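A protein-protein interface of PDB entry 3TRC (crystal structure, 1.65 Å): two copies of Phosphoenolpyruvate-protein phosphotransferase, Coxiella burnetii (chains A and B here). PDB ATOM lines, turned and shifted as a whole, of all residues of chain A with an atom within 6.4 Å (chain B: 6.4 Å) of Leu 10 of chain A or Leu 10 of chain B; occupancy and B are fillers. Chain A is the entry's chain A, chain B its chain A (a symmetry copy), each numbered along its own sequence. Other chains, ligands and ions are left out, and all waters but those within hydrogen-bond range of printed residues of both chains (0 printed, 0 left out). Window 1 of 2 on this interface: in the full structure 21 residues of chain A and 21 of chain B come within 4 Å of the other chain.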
ATOM      1  N   ASN A   5     -15.207  14.233 -30.651  1.00  0.00           N
ATOM      2  CA  ASN A   5     -15.181  12.905 -30.038  1.00  0.00           C
ATOM      3  C   ASN A   5     -16.382  12.681 -29.131  1.00  0.00           C
ATOM      4  O   ASN A   5     -17.066  11.665 -29.232  1.00  0.00           O
ATOM      5  CB  ASN A   5     -13.903  12.703 -29.227  1.00  0.00           C
ATOM      6  CG  ASN A   5     -12.704  12.434 -30.096  1.00  0.00           C
ATOM      7  OD1 ASN A   5     -11.806  13.264 -30.200  1.00  0.00           O
ATOM      8  ND2 ASN A   5     -12.674  11.264 -30.722  1.00  0.00           N
ATOM      9  N   MET A   6     -16.631  13.633 -28.239  1.00  0.00           N
ATOM     10  CA  MET A   6     -17.767  13.543 -27.329  1.00  0.00           C
ATOM     11  C   MET A   6     -19.040  13.236 -28.101  1.00  0.00           C
ATOM     12  O   MET A   6     -19.846  12.400 -27.703  1.00  0.00           O
ATOM     13  CB  MET A   6     -17.934  14.850 -26.551  1.00  0.00           C
ATOM     14  CG  MET A   6     -16.767  15.187 -25.663  1.00  0.00           C
ATOM     15  SD  MET A   6     -16.515  13.818 -24.311  1.00  0.00           S
ATOM     16  CE  MET A   6     -14.907  13.003 -24.984  1.00  0.00           C
ATOM     17  N   LEU A   7     -19.217  13.928 -29.218  1.00  0.00           N
ATOM     18  CA  LEU A   7     -20.402  13.768 -30.033  1.00  0.00           C
ATOM     19  C   LEU A   7     -20.567  12.330 -30.533  1.00  0.00           C
ATOM     20  O   LEU A   7     -21.653  11.762 -30.476  1.00  0.00           O
ATOM     21  CB  LEU A   7     -20.316  14.737 -31.207  1.00  0.00           C
ATOM     22  CG  LEU A   7     -21.582  15.125 -31.941  1.00  0.00           C
ATOM     23  CD1 LEU A   7     -22.698  15.529 -30.972  1.00  0.00           C
ATOM     24  CD2 LEU A   7     -21.228  16.263 -32.880  1.00  0.00           C
ATOM     25  N   LYS A   8     -19.478  11.736 -31.004  1.00  0.00           N
ATOM     26  CA  LYS A   8     -19.528  10.373 -31.516  1.00  0.00           C
ATOM     27  C   LYS A   8     -19.613   9.335 -30.398  1.00  0.00           C
ATOM     28  O   LYS A   8     -20.195   8.264 -30.575  1.00  0.00           O
ATOM     29  CB  LYS A   8     -18.322  10.099 -32.408  1.00  0.00           C
ATOM     30  CG  LYS A   8     -18.269  10.980 -33.637  1.00  0.00           C
ATOM     31  CD  LYS A   8     -17.061  10.643 -34.475  1.00  0.00           C
ATOM     32  CE  LYS A   8     -16.990  11.511 -35.716  1.00  0.00           C
ATOM     33  NZ  LYS A   8     -15.610  11.516 -36.272  1.00  0.00           N
ATOM     34  N   ILE A   9     -19.026   9.650 -29.250  1.00  0.00           N
ATOM     35  CA  ILE A   9     -19.146   8.783 -28.085  1.00  0.00           C
ATOM     36  C   ILE A   9     -20.599   8.752 -27.646  1.00  0.00           C
ATOM     37  O   ILE A   9     -21.142   7.694 -27.340  1.00  0.00           O
ATOM     38  CB  ILE A   9     -18.279   9.278 -26.919  1.00  0.00           C
ATOM     39  CG1 ILE A   9     -16.803   9.163 -27.288  1.00  0.00           C
ATOM     40  CG2 ILE A   9     -18.593   8.493 -25.634  1.00  0.00           C
ATOM     41  CD1 ILE A   9     -15.884   9.968 -26.404  1.00  0.00           C
ATOM     42  N   LEU A  10     -21.218   9.927 -27.625  1.00  0.00           N
ATOM     43  CA  LEU A  10     -22.626  10.047 -27.285  1.00  0.00           C
ATOM     44  C   LEU A  10     -23.438   9.187 -28.234  1.00  0.00           C
ATOM     45  O   LEU A  10     -24.362   8.486 -27.830  1.00  0.00           O
ATOM     46  CB  LEU A  10     -23.081  11.500 -27.405  1.00  0.00           C
ATOM     47  CG  LEU A  10     -23.399  12.260 -26.127  1.00  0.00           C
ATOM     48  CD1 LEU A  10     -24.172  13.525 -26.471  1.00  0.00           C
ATOM     49  CD2 LEU A  10     -24.199  11.380 -25.165  1.00  0.00           C
ATOM     50  N   ARG A  11     -23.083   9.247 -29.512  1.00  0.00           N
ATOM     51  CA  ARG A  11     -23.780   8.476 -30.527  1.00  0.00           C
ATOM     52  C   ARG A  11     -23.744   6.986 -30.190  1.00  0.00           C
ATOM     53  O   ARG A  11     -24.775   6.317 -30.189  1.00  0.00           O
ATOM     54  CB  ARG A  11     -23.144   8.733 -31.893  1.00  0.00           C
ATOM     55  CG  ARG A  11     -23.924   8.199 -33.077  1.00  0.00           C
ATOM     56  CD  ARG A  11     -23.095   8.343 -34.344  1.00  0.00           C
ATOM     57  NE  ARG A  11     -21.819   7.638 -34.235  1.00  0.00           N
ATOM     58  CZ  ARG A  11     -20.734   7.938 -34.942  1.00  0.00           C
ATOM     59  NH1 ARG A  11     -20.762   8.938 -35.811  1.00  0.00           N
ATOM     60  NH2 ARG A  11     -19.616   7.241 -34.776  1.00  0.00           N
ATOM     61  N   GLN A  12     -22.552   6.478 -29.885  1.00  0.00           N
ATOM     62  CA  GLN A  12     -22.365   5.060 -29.590  1.00  0.00           C
ATOM     63  C   GLN A  12     -23.021   4.627 -28.276  1.00  0.00           C
ATOM     64  O   GLN A  12     -23.649   3.568 -28.213  1.00  0.00           O
ATOM     65  CB  GLN A  12     -20.872   4.702 -29.583  1.00  0.00           C
ATOM     66  CG  GLN A  12     -20.550   3.309 -29.039  1.00  0.00           C
ATOM     67  CD  GLN A  12     -20.914   2.183 -30.001  1.00  0.00           C
ATOM     68  OE1 GLN A  12     -21.162   2.413 -31.186  1.00  0.00           O
ATOM     69  NE2 GLN A  12     -20.942   0.957 -29.490  1.00  0.00           N
ATOM     70  N   ILE A  13     -22.878   5.439 -27.231  1.00  0.00           N
ATOM     71  CA  ILE A  13     -23.433   5.078 -25.930  1.00  0.00           C
ATOM     72  C   ILE A  13     -24.954   5.227 -25.876  1.00  0.00           C
ATOM     73  O   ILE A  13     -25.629   4.453 -25.204  1.00  0.00           O
ATOM     74  CB  ILE A  13     -22.785   5.868 -24.776  1.00  0.00           C
ATOM     75  CG1 ILE A  13     -23.215   5.291 -23.431  1.00  0.00           C
ATOM     76  CG2 ILE A  13     -23.155   7.344 -24.853  1.00  0.00           C
ATOM     77  CD1 ILE A  13     -22.425   5.835 -22.264  1.00  0.00           C
ATOM     78  N   THR A  14     -25.489   6.222 -26.577  1.00  0.00           N
ATOM     79  CA  THR A  14     -26.936   6.418 -26.633  1.00  0.00           C
ATOM     80  C   THR A  14     -27.529   5.166 -27.270  1.00  0.00           C
ATOM     81  O   THR A  14     -28.555   4.648 -26.828  1.00  0.00           O
ATOM     82  CB  THR A  14     -27.316   7.674 -27.447  1.00  0.00           C
ATOM     83  OG1 THR A  14     -26.668   8.824 -26.882  1.00  0.00           O
ATOM     84  CG2 THR A  14     -28.822   7.900 -27.423  1.00  0.00           C
ATOM     85  N   GLN A  15     -26.845   4.683 -28.304  1.00  0.00           N
ATOM     86  CA  GLN A  15     -27.181   3.433 -28.975  1.00  0.00           C
ATOM     87  C   GLN A  15     -27.180   2.258 -28.004  1.00  0.00           C
ATOM     88  O   GLN A  15     -28.147   1.500 -27.924  1.00  0.00           O
ATOM     89  CB  GLN A  15     -26.163   3.157 -30.081  1.00  0.00           C
ATOM     90  CG  GLN A  15     -26.448   1.918 -30.896  1.00  0.00           C
ATOM     91  CD  GLN A  15     -27.374   2.204 -32.055  1.00  0.00           C
ATOM     92  OE1 GLN A  15     -28.593   2.255 -31.890  1.00  0.00           O
ATOM     93  NE2 GLN A  15     -26.800   2.406 -33.235  1.00  0.00           N
ATOM     94  N   ALA A 146     -20.582  18.856 -20.794  1.00  0.00           N
ATOM     95  CA  ALA A 146     -21.749  18.858 -21.676  1.00  0.00           C
ATOM     96  C   ALA A 146     -22.146  17.435 -22.072  1.00  0.00           C
ATOM     97  O   ALA A 146     -23.329  17.081 -22.094  1.00  0.00           O
ATOM     98  CB  ALA A 146     -21.475  19.707 -22.913  1.00  0.00           C
ATOM     99  N   PHE A 147     -21.150  16.619 -22.382  1.00  0.00           N
ATOM    100  CA  PHE A 147     -21.369  15.217 -22.693  1.00  0.00           C
ATOM    101  C   PHE A 147     -22.047  14.493 -21.534  1.00  0.00           C
ATOM    102  O   PHE A 147     -23.058  13.813 -21.712  1.00  0.00           O
ATOM    103  CB  PHE A 147     -20.034  14.549 -23.003  1.00  0.00           C
ATOM    104  CG  PHE A 147     -20.106  13.061 -23.066  1.00  0.00           C
ATOM    105  CD1 PHE A 147     -20.588  12.426 -24.194  1.00  0.00           C
ATOM    106  CD2 PHE A 147     -19.692  12.295 -21.993  1.00  0.00           C
ATOM    107  CE1 PHE A 147     -20.656  11.054 -24.249  1.00  0.00           C
ATOM    108  CE2 PHE A 147     -19.759  10.928 -22.047  1.00  0.00           C
ATOM    109  CZ  PHE A 147     -20.239  10.304 -23.171  1.00  0.00           C
ATOM    110  N   THR A 150     -25.665  15.825 -20.860  1.00  0.00           N
ATOM    111  CA  THR A 150     -26.573  15.341 -21.888  1.00  0.00           C
ATOM    112  C   THR A 150     -26.894  13.874 -21.647  1.00  0.00           C
ATOM    113  O   THR A 150     -28.050  13.447 -21.769  1.00  0.00           O
ATOM    114  CB  THR A 150     -25.966  15.542 -23.300  1.00  0.00           C
ATOM    115  OG1 THR A 150     -25.685  16.932 -23.489  1.00  0.00           O
ATOM    116  CG2 THR A 150     -26.940  15.089 -24.367  1.00  0.00           C
ATOM    117  N   LEU A 151     -25.877  13.107 -21.273  1.00  0.00           N
ATOM    118  CA  LEU A 151     -26.046  11.697 -20.947  1.00  0.00           C
ATOM    119  C   LEU A 151     -26.975  11.493 -19.745  1.00  0.00           C
ATOM    120  O   LEU A 151     -27.824  10.599 -19.752  1.00  0.00           O
ATOM    121  CB  LEU A 151     -24.689  11.065 -20.666  1.00  0.00           C
ATOM    122  CG  LEU A 151     -24.665   9.569 -20.366  1.00  0.00           C
ATOM    123  CD1 LEU A 151     -25.259   8.788 -21.531  1.00  0.00           C
ATOM    124  CD2 LEU A 151     -23.246   9.114 -20.076  1.00  0.00           C
ATOM    125  N   ILE A 153     -29.438  13.180 -18.790  1.00  0.00           N
ATOM    126  CA  ILE A 153     -30.832  13.341 -19.190  1.00  0.00           C
ATOM    127  C   ILE A 153     -31.389  11.996 -19.642  1.00  0.00           C
ATOM    128  O   ILE A 153     -32.518  11.632 -19.315  1.00  0.00           O
ATOM    129  CB  ILE A 153     -30.973  14.381 -20.312  1.00  0.00           C
ATOM    130  CG1 ILE A 153     -30.452  15.732 -19.815  1.00  0.00           C
ATOM    131  CG2 ILE A 153     -32.420  14.487 -20.769  1.00  0.00           C
ATOM    132  CD1 ILE A 153     -30.326  16.785 -20.883  1.00  0.00           C
ATOM    133  N   ASN B   5     -21.044  23.307 -30.339  1.00  0.00           N
ATOM    134  CA  ASN B   5     -22.440  23.735 -30.425  1.00  0.00           C
ATOM    135  C   ASN B   5     -23.389  22.549 -30.505  1.00  0.00           C
ATOM    136  O   ASN B   5     -24.366  22.474 -29.765  1.00  0.00           O
ATOM    137  CB  ASN B   5     -22.663  24.631 -31.642  1.00  0.00           C
ATOM    138  CG  ASN B   5     -22.142  26.028 -31.435  1.00  0.00           C
ATOM    139  OD1 ASN B   5     -21.163  26.431 -32.054  1.00  0.00           O
ATOM    140  ND2 ASN B   5     -22.803  26.785 -30.566  1.00  0.00           N
ATOM    141  N   MET B   6     -23.098  21.624 -31.413  1.00  0.00           N
ATOM    142  CA  MET B   6     -23.919  20.429 -31.569  1.00  0.00           C
ATOM    143  C   MET B   6     -24.138  19.758 -30.224  1.00  0.00           C
ATOM    144  O   MET B   6     -25.242  19.339 -29.887  1.00  0.00           O
ATOM    145  CB  MET B   6     -23.256  19.448 -32.539  1.00  0.00           C
ATOM    146  CG  MET B   6     -23.098  19.981 -33.937  1.00  0.00           C
ATOM    147  SD  MET B   6     -24.828  20.379 -34.719  1.00  0.00           S
ATOM    148  CE  MET B   6     -24.749  22.302 -34.696  1.00  0.00           C
ATOM    149  N   LEU B   7     -23.065  19.653 -29.451  1.00  0.00           N
ATOM    150  CA  LEU B   7     -23.117  19.001 -28.161  1.00  0.00           C
ATOM    151  C   LEU B   7     -24.113  19.677 -27.214  1.00  0.00           C
ATOM    152  O   LEU B   7     -24.902  19.014 -26.549  1.00  0.00           O
ATOM    153  CB  LEU B   7     -21.716  19.008 -27.559  1.00  0.00           C
ATOM    154  CG  LEU B   7     -21.373  18.014 -26.470  1.00  0.00           C
ATOM    155  CD1 LEU B   7     -21.807  16.593 -26.841  1.00  0.00           C
ATOM    156  CD2 LEU B   7     -19.875  18.092 -26.243  1.00  0.00           C
ATOM    157  N   LYS B   8     -24.087  21.003 -27.172  1.00  0.00           N
ATOM    158  CA  LYS B   8     -24.984  21.745 -26.295  1.00  0.00           C
ATOM    159  C   LYS B   8     -26.415  21.787 -26.830  1.00  0.00           C
ATOM    160  O   LYS B   8     -27.374  21.847 -26.059  1.00  0.00           O
ATOM    161  CB  LYS B   8     -24.456  23.157 -26.071  1.00  0.00           C
ATOM    162  CG  LYS B   8     -23.110  23.194 -25.380  1.00  0.00           C
ATOM    163  CD  LYS B   8     -22.659  24.620 -25.180  1.00  0.00           C
ATOM    164  CE  LYS B   8     -21.314  24.682 -24.484  1.00  0.00           C
ATOM    165  NZ  LYS B   8     -20.671  26.004 -24.707  1.00  0.00           N
ATOM    166  N   ILE B   9     -26.556  21.766 -28.150  1.00  0.00           N
ATOM    167  CA  ILE B   9     -27.876  21.686 -28.760  1.00  0.00           C
ATOM    168  C   ILE B   9     -28.503  20.352 -28.399  1.00  0.00           C
ATOM    169  O   ILE B   9     -29.678  20.283 -28.044  1.00  0.00           O
ATOM    170  CB  ILE B   9     -27.802  21.809 -30.289  1.00  0.00           C
ATOM    171  CG1 ILE B   9     -27.325  23.207 -30.671  1.00  0.00           C
ATOM    172  CG2 ILE B   9     -29.165  21.494 -30.928  1.00  0.00           C
ATOM    173  CD1 ILE B   9     -26.841  23.322 -32.095  1.00  0.00           C
ATOM    174  N   LEU B  10     -27.702  19.297 -28.490  1.00  0.00           N
ATOM    175  CA  LEU B  10     -28.142  17.962 -28.118  1.00  0.00           C
ATOM    176  C   LEU B  10     -28.612  17.982 -26.676  1.00  0.00           C
ATOM    177  O   LEU B  10     -29.638  17.403 -26.330  1.00  0.00           O
ATOM    178  CB  LEU B  10     -26.998  16.963 -28.264  1.00  0.00           C
ATOM    179  CG  LEU B  10     -27.074  15.944 -29.391  1.00  0.00           C
ATOM    180  CD1 LEU B  10     -26.060  14.838 -29.139  1.00  0.00           C
ATOM    181  CD2 LEU B  10     -28.487  15.371 -29.501  1.00  0.00           C
ATOM    182  N   ARG B  11     -27.845  18.659 -25.830  1.00  0.00           N
ATOM    183  CA  ARG B  11     -28.177  18.754 -24.420  1.00  0.00           C
ATOM    184  C   ARG B  11     -29.571  19.353 -24.234  1.00  0.00           C
ATOM    185  O   ARG B  11     -30.402  18.799 -23.518  1.00  0.00           O
ATOM    186  CB  ARG B  11     -27.127  19.603 -23.702  1.00  0.00           C
ATOM    187  CG  ARG B  11     -27.203  19.576 -22.189  1.00  0.00           C
ATOM    188  CD  ARG B  11     -26.244  20.605 -21.609  1.00  0.00           C
ATOM    189  NE  ARG B  11     -26.543  21.951 -22.094  1.00  0.00           N
ATOM    190  CZ  ARG B  11     -25.660  22.944 -22.145  1.00  0.00           C
ATOM    191  NH1 ARG B  11     -24.412  22.744 -21.746  1.00  0.00           N
ATOM    192  NH2 ARG B  11     -26.023  24.137 -22.601  1.00  0.00           N
ATOM    193  N   GLN B  12     -29.824  20.477 -24.900  1.00  0.00           N
ATOM    194  CA  GLN B  12     -31.097  21.182 -24.778  1.00  0.00           C
ATOM    195  C   GLN B  12     -32.273  20.413 -25.386  1.00  0.00           C
ATOM    196  O   GLN B  12     -33.351  20.351 -24.793  1.00  0.00           O
ATOM    197  CB  GLN B  12     -30.999  22.583 -25.396  1.00  0.00           C
ATOM    198  CG  GLN B  12     -32.337  23.311 -25.549  1.00  0.00           C
ATOM    199  CD  GLN B  12     -32.901  23.827 -24.230  1.00  0.00           C
ATOM    200  OE1 GLN B  12     -32.199  23.895 -23.220  1.00  0.00           O
ATOM    201  NE2 GLN B  12     -34.177  24.196 -24.239  1.00  0.00           N
ATOM    202  N   ILE B  13     -32.067  19.829 -26.565  1.00  0.00           N
ATOM    203  CA  ILE B  13     -33.151  19.115 -27.236  1.00  0.00           C
ATOM    204  C   ILE B  13     -33.458  17.765 -26.586  1.00  0.00           C
ATOM    205  O   ILE B  13     -34.609  17.341 -26.555  1.00  0.00           O
ATOM    206  CB  ILE B  13     -32.883  18.926 -28.742  1.00  0.00           C
ATOM    207  CG1 ILE B  13     -34.133  18.400 -29.440  1.00  0.00           C
ATOM    208  CG2 ILE B  13     -31.717  17.972 -28.972  1.00  0.00           C
ATOM    209  CD1 ILE B  13     -34.039  18.436 -30.948  1.00  0.00           C
ATOM    210  N   THR B  14     -32.432  17.093 -26.075  1.00  0.00           N
ATOM    211  CA  THR B  14     -32.628  15.819 -25.386  1.00  0.00           C
ATOM    212  C   THR B  14     -33.516  16.098 -24.179  1.00  0.00           C
ATOM    213  O   THR B  14     -34.436  15.339 -23.872  1.00  0.00           O
ATOM    214  CB  THR B  14     -31.288  15.192 -24.941  1.00  0.00           C
ATOM    215  OG1 THR B  14     -30.434  15.029 -26.084  1.00  0.00           O
ATOM    216  CG2 THR B  14     -31.513  13.830 -24.299  1.00  0.00           C
ATOM    217  N   GLN B  15     -33.231  17.217 -23.518  1.00  0.00           N
ATOM    218  CA  GLN B  15     -34.033  17.720 -22.409  1.00  0.00           C
ATOM    219  C   GLN B  15     -35.483  17.944 -22.822  1.00  0.00           C
ATOM    220  O   GLN B  15     -36.410  17.459 -22.173  1.00  0.00           O
ATOM    221  CB  GLN B  15     -33.452  19.046 -21.918  1.00  0.00           C
ATOM    222  CG  GLN B  15     -34.161  19.632 -20.721  1.00  0.00           C
ATOM    223  CD  GLN B  15     -33.606  19.103 -19.419  1.00  0.00           C
ATOM    224  OE1 GLN B  15     -33.968  18.014 -18.975  1.00  0.00           O
ATOM    225  NE2 GLN B  15     -32.709  19.867 -18.805  1.00  0.00           N
ATOM    226  N   ALA B 146     -23.438  13.584 -37.207  1.00  0.00           N
ATOM    227  CA  ALA B 146     -23.317  12.896 -35.922  1.00  0.00           C
ATOM    228  C   ALA B 146     -24.413  13.338 -34.951  1.00  0.00           C
ATOM    229  O   ALA B 146     -25.012  12.523 -34.244  1.00  0.00           O
ATOM    230  CB  ALA B 146     -21.935  13.133 -35.322  1.00  0.00           C
ATOM    231  N   PHE B 147     -24.675  14.637 -34.924  1.00  0.00           N
ATOM    232  CA  PHE B 147     -25.748  15.191 -34.116  1.00  0.00           C
ATOM    233  C   PHE B 147     -27.095  14.585 -34.496  1.00  0.00           C
ATOM    234  O   PHE B 147     -27.843  14.110 -33.641  1.00  0.00           O
ATOM    235  CB  PHE B 147     -25.796  16.703 -34.301  1.00  0.00           C
ATOM    236  CG  PHE B 147     -27.022  17.339 -33.739  1.00  0.00           C
ATOM    237  CD1 PHE B 147     -27.129  17.588 -32.384  1.00  0.00           C
ATOM    238  CD2 PHE B 147     -28.071  17.688 -34.567  1.00  0.00           C
ATOM    239  CE1 PHE B 147     -28.261  18.172 -31.868  1.00  0.00           C
ATOM    240  CE2 PHE B 147     -29.199  18.270 -34.053  1.00  0.00           C
ATOM    241  CZ  PHE B 147     -29.298  18.515 -32.706  1.00  0.00           C
ATOM    242  N   THR B 150     -27.280  10.756 -33.705  1.00  0.00           N
ATOM    243  CA  THR B 150     -27.424  10.550 -32.273  1.00  0.00           C
ATOM    244  C   THR B 150     -28.847  10.872 -31.843  1.00  0.00           C
ATOM    245  O   THR B 150     -29.451  10.144 -31.044  1.00  0.00           O
ATOM    246  CB  THR B 150     -26.406  11.415 -31.486  1.00  0.00           C
ATOM    247  OG1 THR B 150     -25.084  11.078 -31.914  1.00  0.00           O
ATOM    248  CG2 THR B 150     -26.523  11.153 -30.000  1.00  0.00           C
ATOM    249  N   LEU B 151     -29.396  11.946 -32.397  1.00  0.00           N
ATOM    250  CA  LEU B 151     -30.772  12.342 -32.129  1.00  0.00           C
ATOM    251  C   LEU B 151     -31.776  11.278 -32.587  1.00  0.00           C
ATOM    252  O   LEU B 151     -32.741  10.980 -31.881  1.00  0.00           O
ATOM    253  CB  LEU B 151     -31.073  13.667 -32.816  1.00  0.00           C
ATOM    254  CG  LEU B 151     -32.457  14.271 -32.593  1.00  0.00           C
ATOM    255  CD1 LEU B 151     -32.696  14.504 -31.106  1.00  0.00           C
ATOM    256  CD2 LEU B 151     -32.598  15.564 -33.374  1.00  0.00           C
ATOM    257  N   ILE B 153     -31.494   8.157 -32.702  1.00  0.00           N
ATOM    258  CA  ILE B 153     -31.538   7.053 -31.750  1.00  0.00           C
ATOM    259  C   ILE B 153     -32.584   7.345 -30.680  1.00  0.00           C
ATOM    260  O   ILE B 153     -33.347   6.467 -30.279  1.00  0.00           O
ATOM    261  CB  ILE B 153     -30.163   6.823 -31.102  1.00  0.00           C
ATOM    262  CG1 ILE B 153     -29.143   6.483 -32.192  1.00  0.00           C
ATOM    263  CG2 ILE B 153     -30.238   5.718 -30.059  1.00  0.00           C
ATOM    264  CD1 ILE B 153     -27.714   6.451 -31.723  1.00  0.00           C
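Of the 16 printed residues of chain A, 9 touch a printed residue of chain B.
Hydrophobic or aromatic side chains of chain B within 4 Å of the printed part of chain A: Met 6, Leu 7, Leu 10, Ala 146 and Ile 153.
Of the printed residues of chain B, Leu 10 of chain A touches Leu 7 and Leu 10.
Gln 12 of chain A touches none of the printed residues of chain B.
Of the printed residues of chain B, Ile 153 of chain A touches Arg 11 (3.3 Å), Thr 14 (3.7 Å) and Gln 15 (3.9 Å).
Of the printed residues of chain A, Thr 14 of chain B touches Thr 150 and Ile 153.
Printed residues of chain A within 4 Å of Gln 15 of chain B: Ile 153 (3.9 Å).
Of the printed residues of chain A, Ala 146 of chain B touches Leu 7.
The nearest residue of chain B that does not touch Leu 10 of chain A is Thr 150 of chain B (4.1 Å).
The nearest residue of chain A that does not touch Leu 10 of chain B is Thr 150 of chain A (4.1 Å).
The nearest printed residue of chain A that does not touch Leu 7 of chain B is Phe 147 of chain A (4.3 Å).
OG1 of Thr 150 of chain B lies within hydrogen-bond range of O of Ala 146 of chain B.
The backbone carbonyl oxygen (O) of Leu 10 of chain B lies within hydrogen-bond range of the side-chain hydroxyl (OG1) of Thr 14 of chain B.
The backbone carbonyl oxygen (O) of Ala 146 of chain A sits at hydrogen-bond distance from the side-chain hydroxyl (OG1) of Thr 150 of chain A, at 2.7 Å.
The backbone carbonyl oxygen of Leu 10 of chain A lies within hydrogen-bond range of the side-chain hydroxyl of Thr 14 of chain A (2.5 Å).
Leu 7 of chain A touches Leu 10 of chain B (CD1 to CD1, 3.9 Å).
Ala 146 of chain B touches Leu 7 of chain A (CB to CG, 3.9 Å).
CD1 of Leu 10 of chain A touches CD1 of Leu 7 of chain B, at 3.9 Å.
Leu 10 of chain A touches Leu 10 of chain B.
Thr 14 of chain A touches Thr 150 of chain B.
Thr 14 of chain A touches Ile 153 of chain B.
Ala 146 of chain A touches Leu 7 of chain B (CB to CG, 3.9 Å).
CB of Arg 11 of chain B touches OG1 of Thr 150 of chain A, at 3.0 Å.
OG1 of Thr 14 of chain B touches CG2 of Thr 150 of chain A (3.9 Å).
Ile 153 of chain A touches Gln 15 of chain B.
Leu 7 of chain A touches Leu 10 of chain B, and with the chains exchanged Leu 10 of chain A touches Leu 7 of chain B.
Leu 7 of chain A touches Thr 150 of chain B, and with the chains exchanged Thr 150 of chain A touches Leu 7 of chain B.
Leu 10 of chain A touches its own counterpart, Leu 10 of chain B.
Thr 14 of chain A touches Ile 153 of chain B, and with the chains exchanged Ile 153 of chain A touches Thr 14 of chain B.
Positions printed for both chains: 5, 6, 7, 8, 9, 10, 11, 12, 13, 14, 15, 146, 147, 150, 151 and 153.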
